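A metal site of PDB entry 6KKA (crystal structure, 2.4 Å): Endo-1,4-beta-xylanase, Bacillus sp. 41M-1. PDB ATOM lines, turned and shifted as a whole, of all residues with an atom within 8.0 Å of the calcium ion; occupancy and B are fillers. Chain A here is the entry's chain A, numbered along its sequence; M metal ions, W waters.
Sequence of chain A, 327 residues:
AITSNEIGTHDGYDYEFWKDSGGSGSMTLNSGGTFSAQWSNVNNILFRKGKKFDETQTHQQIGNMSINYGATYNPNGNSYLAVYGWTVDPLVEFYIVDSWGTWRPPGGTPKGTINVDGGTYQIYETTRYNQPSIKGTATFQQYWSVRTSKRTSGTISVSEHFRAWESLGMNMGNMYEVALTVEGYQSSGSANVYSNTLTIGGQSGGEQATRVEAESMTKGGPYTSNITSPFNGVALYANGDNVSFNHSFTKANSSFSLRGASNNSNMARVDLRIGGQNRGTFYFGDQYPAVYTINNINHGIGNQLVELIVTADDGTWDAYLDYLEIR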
ATOM      1  N   TYR A 223      15.632 -19.582  32.073  1.00  0.00           N
ATOM      2  CA  TYR A 223      14.570 -20.186  31.275  1.00  0.00           C
ATOM      3  C   TYR A 223      15.008 -21.036  30.093  1.00  0.00           C
ATOM      4  O   TYR A 223      14.143 -21.653  29.460  1.00  0.00           O
ATOM      5  CB  TYR A 223      13.631 -19.092  30.755  1.00  0.00           C
ATOM      6  CG  TYR A 223      13.031 -18.261  31.849  1.00  0.00           C
ATOM      7  CD1 TYR A 223      12.144 -18.821  32.770  1.00  0.00           C
ATOM      8  CD2 TYR A 223      13.353 -16.929  31.988  1.00  0.00           C
ATOM      9  CE1 TYR A 223      11.591 -18.049  33.796  1.00  0.00           C
ATOM     10  CE2 TYR A 223      12.814 -16.155  32.992  1.00  0.00           C
ATOM     11  CZ  TYR A 223      11.933 -16.721  33.893  1.00  0.00           C
ATOM     12  OH  TYR A 223      11.400 -15.927  34.889  1.00  0.00           O
ATOM     13  N   LEU A 236      16.601 -18.872  24.111  1.00  0.00           N
ATOM     14  CA  LEU A 236      17.113 -18.031  25.200  1.00  0.00           C
ATOM     15  C   LEU A 236      16.096 -16.927  25.401  1.00  0.00           C
ATOM     16  O   LEU A 236      15.898 -16.080  24.519  1.00  0.00           O
ATOM     17  CB  LEU A 236      18.505 -17.481  24.873  1.00  0.00           C
ATOM     18  CG  LEU A 236      19.537 -18.483  24.321  1.00  0.00           C
ATOM     19  CD1 LEU A 236      20.881 -17.815  24.034  1.00  0.00           C
ATOM     20  CD2 LEU A 236      19.733 -19.686  25.254  1.00  0.00           C
ATOM     21  N   TYR A 237      15.447 -16.911  26.563  1.00  0.00           N
ATOM     22  CA  TYR A 237      14.311 -16.030  26.757  1.00  0.00           C
ATOM     23  C   TYR A 237      14.648 -14.778  27.554  1.00  0.00           C
ATOM     24  O   TYR A 237      14.046 -13.735  27.307  1.00  0.00           O
ATOM     25  CB  TYR A 237      13.171 -16.757  27.493  1.00  0.00           C
ATOM     26  CG  TYR A 237      12.681 -18.020  26.821  1.00  0.00           C
ATOM     27  CD1 TYR A 237      11.600 -17.982  25.932  1.00  0.00           C
ATOM     28  CD2 TYR A 237      13.276 -19.249  27.102  1.00  0.00           C
ATOM     29  CE1 TYR A 237      11.136 -19.139  25.323  1.00  0.00           C
ATOM     30  CE2 TYR A 237      12.805 -20.413  26.507  1.00  0.00           C
ATOM     31  CZ  TYR A 237      11.736 -20.358  25.617  1.00  0.00           C
ATOM     32  OH  TYR A 237      11.288 -21.512  25.023  1.00  0.00           O
ATOM     33  N   ALA A 238      15.564 -14.848  28.506  1.00  0.00           N
ATOM     34  CA  ALA A 238      15.782 -13.727  29.422  1.00  0.00           C
ATOM     35  C   ALA A 238      17.275 -13.459  29.539  1.00  0.00           C
ATOM     36  O   ALA A 238      18.106 -14.271  29.122  1.00  0.00           O
ATOM     37  CB  ALA A 238      15.160 -14.028  30.799  1.00  0.00           C
ATOM     38  N   ASN A 239      17.608 -12.313  30.119  1.00  0.00           N
ATOM     39  CA  ASN A 239      19.017 -12.007  30.346  1.00  0.00           C
ATOM     40  C   ASN A 239      19.641 -13.038  31.271  1.00  0.00           C
ATOM     41  O   ASN A 239      19.044 -13.449  32.269  1.00  0.00           O
ATOM     42  CB  ASN A 239      19.150 -10.598  30.912  1.00  0.00           C
ATOM     43  CG  ASN A 239      18.929  -9.554  29.843  1.00  0.00           C
ATOM     44  OD1 ASN A 239      19.233  -9.811  28.681  1.00  0.00           O
ATOM     45  ND2 ASN A 239      18.390  -8.409  30.217  1.00  0.00           N
ATOM     46  N   ASP A 241      20.152 -16.136  30.212  1.00  0.00           N
ATOM     47  CA  ASP A 241      19.953 -17.401  29.519  1.00  0.00           C
ATOM     48  C   ASP A 241      21.137 -17.636  28.604  1.00  0.00           C
ATOM     49  O   ASP A 241      21.538 -16.745  27.840  1.00  0.00           O
ATOM     50  CB  ASP A 241      18.666 -17.401  28.705  1.00  0.00           C
ATOM     51  CG  ASP A 241      17.463 -17.845  29.505  1.00  0.00           C
ATOM     52  OD1 ASP A 241      17.623 -18.254  30.687  1.00  0.00           O
ATOM     53  OD2 ASP A 241      16.360 -17.797  28.928  1.00  0.00           O
ATOM     54  N   ASN A 263      12.464 -14.891  17.489  1.00  0.00           N
ATOM     55  CA  ASN A 263      11.143 -15.487  17.406  1.00  0.00           C
ATOM     56  C   ASN A 263      10.183 -14.635  16.589  1.00  0.00           C
ATOM     57  O   ASN A 263       9.109 -15.111  16.219  1.00  0.00           O
ATOM     58  CB  ASN A 263      10.548 -15.733  18.786  1.00  0.00           C
ATOM     59  CG  ASN A 263      10.196 -14.453  19.480  1.00  0.00           C
ATOM     60  OD1 ASN A 263      10.957 -13.496  19.412  1.00  0.00           O
ATOM     61  ND2 ASN A 263       9.043 -14.421  20.140  1.00  0.00           N
ATOM     62  N   ASN A 264      10.540 -13.390  16.262  1.00  0.00           N
ATOM     63  CA  ASN A 264       9.596 -12.505  15.600  1.00  0.00           C
ATOM     64  C   ASN A 264      10.375 -11.560  14.701  1.00  0.00           C
ATOM     65  O   ASN A 264      11.542 -11.821  14.386  1.00  0.00           O
ATOM     66  CB  ASN A 264       8.725 -11.785  16.657  1.00  0.00           C
ATOM     67  CG  ASN A 264       9.563 -10.984  17.660  1.00  0.00           C
ATOM     68  OD1 ASN A 264      10.619 -10.417  17.328  1.00  0.00           O
ATOM     69  ND2 ASN A 264       9.089 -10.948  18.891  1.00  0.00           N
ATOM     70  N   VAL A 310      22.326 -14.390  26.114  1.00  0.00           N
ATOM     71  CA  VAL A 310      21.494 -13.215  25.936  1.00  0.00           C
ATOM     72  C   VAL A 310      21.772 -12.241  27.072  1.00  0.00           C
ATOM     73  O   VAL A 310      21.687 -12.596  28.251  1.00  0.00           O
ATOM     74  CB  VAL A 310      20.005 -13.600  25.910  1.00  0.00           C
ATOM     75  CG1 VAL A 310      19.125 -12.388  26.238  1.00  0.00           C
ATOM     76  CG2 VAL A 310      19.634 -14.143  24.536  1.00  0.00           C
ATOM     77  N   ALA A 312      20.840  -8.523  26.345  1.00  0.00           N
ATOM     78  CA  ALA A 312      20.113  -7.293  26.039  1.00  0.00           C
ATOM     79  C   ALA A 312      18.611  -7.535  25.863  1.00  0.00           C
ATOM     80  O   ALA A 312      17.941  -6.772  25.169  1.00  0.00           O
ATOM     81  CB  ALA A 312      20.688  -6.616  24.805  1.00  0.00           C
ATOM     82  N   ASP A 313      18.088  -8.582  26.470  1.00  0.00           N
ATOM     83  CA  ASP A 313      16.656  -8.853  26.387  1.00  0.00           C
ATOM     84  C   ASP A 313      15.879  -7.725  27.045  1.00  0.00           C
ATOM     85  O   ASP A 313      16.332  -7.151  28.043  1.00  0.00           O
ATOM     86  CB  ASP A 313      16.317 -10.160  27.086  1.00  0.00           C
ATOM     87  CG  ASP A 313      14.817 -10.335  27.266  1.00  0.00           C
ATOM     88  OD1 ASP A 313      14.137 -10.591  26.266  1.00  0.00           O
ATOM     89  OD2 ASP A 313      14.309 -10.173  28.402  1.00  0.00           O
ATOM     90  N   ASP A 314      14.695  -7.408  26.475  1.00  0.00           N
ATOM     91  CA  ASP A 314      13.758  -6.477  27.113  1.00  0.00           C
ATOM     92  C   ASP A 314      12.310  -6.933  26.956  1.00  0.00           C
ATOM     93  O   ASP A 314      11.407  -6.102  27.072  1.00  0.00           O
ATOM     94  CB  ASP A 314      13.879  -5.040  26.577  1.00  0.00           C
ATOM     95  CG  ASP A 314      13.709  -4.955  25.058  1.00  0.00           C
ATOM     96  OD1 ASP A 314      13.239  -5.929  24.436  1.00  0.00           O
ATOM     97  OD2 ASP A 314      14.049  -3.893  24.493  1.00  0.00           O
ATOM     98  N   GLY A 315      12.071  -8.206  26.682  1.00  0.00           N
ATOM     99  CA  GLY A 315      10.738  -8.741  26.491  1.00  0.00           C
ATOM    100  C   GLY A 315      10.164  -8.622  25.096  1.00  0.00           C
ATOM    101  O   GLY A 315       9.011  -9.002  24.881  1.00  0.00           O
ATOM    102  N   THR A 316      10.922  -8.088  24.125  1.00  0.00           N
ATOM    103  CA  THR A 316      10.388  -7.908  22.791  1.00  0.00           C
ATOM    104  C   THR A 316      10.850  -8.955  21.795  1.00  0.00           C
ATOM    105  O   THR A 316      10.466  -8.889  20.619  1.00  0.00           O
ATOM    106  CB  THR A 316      10.735  -6.500  22.267  1.00  0.00           C
ATOM    107  OG1 THR A 316      12.154  -6.339  22.176  1.00  0.00           O
ATOM    108  CG2 THR A 316      10.132  -5.424  23.192  1.00  0.00           C
ATOM    109  N   TRP A 317      11.663  -9.923  22.221  1.00  0.00           N
ATOM    110  CA  TRP A 317      12.131 -10.992  21.328  1.00  0.00           C
ATOM    111  C   TRP A 317      12.727 -12.092  22.194  1.00  0.00           C
ATOM    112  O   TRP A 317      13.143 -11.846  23.318  1.00  0.00           O
ATOM    113  CB  TRP A 317      13.172 -10.503  20.312  1.00  0.00           C
ATOM    114  CG  TRP A 317      14.341  -9.741  20.908  1.00  0.00           C
ATOM    115  CD1 TRP A 317      14.449  -8.377  21.027  1.00  0.00           C
ATOM    116  CD2 TRP A 317      15.552 -10.281  21.460  1.00  0.00           C
ATOM    117  NE1 TRP A 317      15.646  -8.042  21.614  1.00  0.00           N
ATOM    118  CE2 TRP A 317      16.343  -9.183  21.886  1.00  0.00           C
ATOM    119  CE3 TRP A 317      16.041 -11.578  21.634  1.00  0.00           C
ATOM    120  CZ2 TRP A 317      17.600  -9.354  22.488  1.00  0.00           C
ATOM    121  CZ3 TRP A 317      17.299 -11.750  22.222  1.00  0.00           C
ATOM    122  CH2 TRP A 317      18.060 -10.633  22.651  1.00  0.00           C
ATOM    123  N   ASP A 318      12.789 -13.282  21.620  1.00  0.00           N
ATOM    124  CA  ASP A 318      13.565 -14.388  22.144  1.00  0.00           C
ATOM    125  C   ASP A 318      14.575 -14.793  21.077  1.00  0.00           C
ATOM    126  O   ASP A 318      14.376 -14.538  19.887  1.00  0.00           O
ATOM    127  CB  ASP A 318      12.695 -15.605  22.501  1.00  0.00           C
ATOM    128  CG  ASP A 318      11.629 -15.297  23.517  1.00  0.00           C
ATOM    129  OD1 ASP A 318      11.877 -14.485  24.419  1.00  0.00           O
ATOM    130  OD2 ASP A 318      10.534 -15.911  23.438  1.00  0.00           O
ATOM    131  N   ALA A 319      15.647 -15.451  21.525  1.00  0.00           N
ATOM    132  CA  ALA A 319      16.704 -15.935  20.663  1.00  0.00           C
ATOM    133  C   ALA A 319      16.563 -17.447  20.521  1.00  0.00           C
ATOM    134  O   ALA A 319      16.468 -18.153  21.530  1.00  0.00           O
ATOM    135  CB  ALA A 319      18.080 -15.574  21.252  1.00  0.00           C
HETATM  136 CA    CA M   1      13.135 -12.615  25.467  1.00  0.00          CA
HETATM  137  O   HOH W   1      15.713 -13.507  24.767  1.00  0.00           O
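Four residues have an atom within 4 Å of the calcium ion: Tyr 237, Asp 313, Trp 317 and Asp 318. The nearest printed residue that does not touch the calcium ion is Ala 238 (4.5 Å).
The calcium ion is bound by O of Trp 317, at 2.3 Å. O of Tyr 237 binds the calcium ion, at 2.3 Å. The side-chain carboxylate (OD1) of Asp 313 binds the calcium ion, at 2.4 Å. The side-chain carboxylate (OD1) of Asp 318 is bound to the calcium ion, at 2.5 Å. The calcium ion is bound by water W1, at 2.8 Å.
N of Asp 318 is in hydrogen-bond range of OD1 of Asn 263, 2.9 Å away. The side-chain carboxylate (OD2) of Asp 313 is in hydrogen-bond range of the backbone NH (N) of Gly 315 (3.4 Å). The backbone NH of Asp 313 sits at hydrogen-bond distance from the side-chain amide oxygen of Asn 239 (2.8 Å). The side-chain carboxylate of Asp 241 sits at hydrogen-bond distance from the backbone NH of Tyr 237 (2.7 Å).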
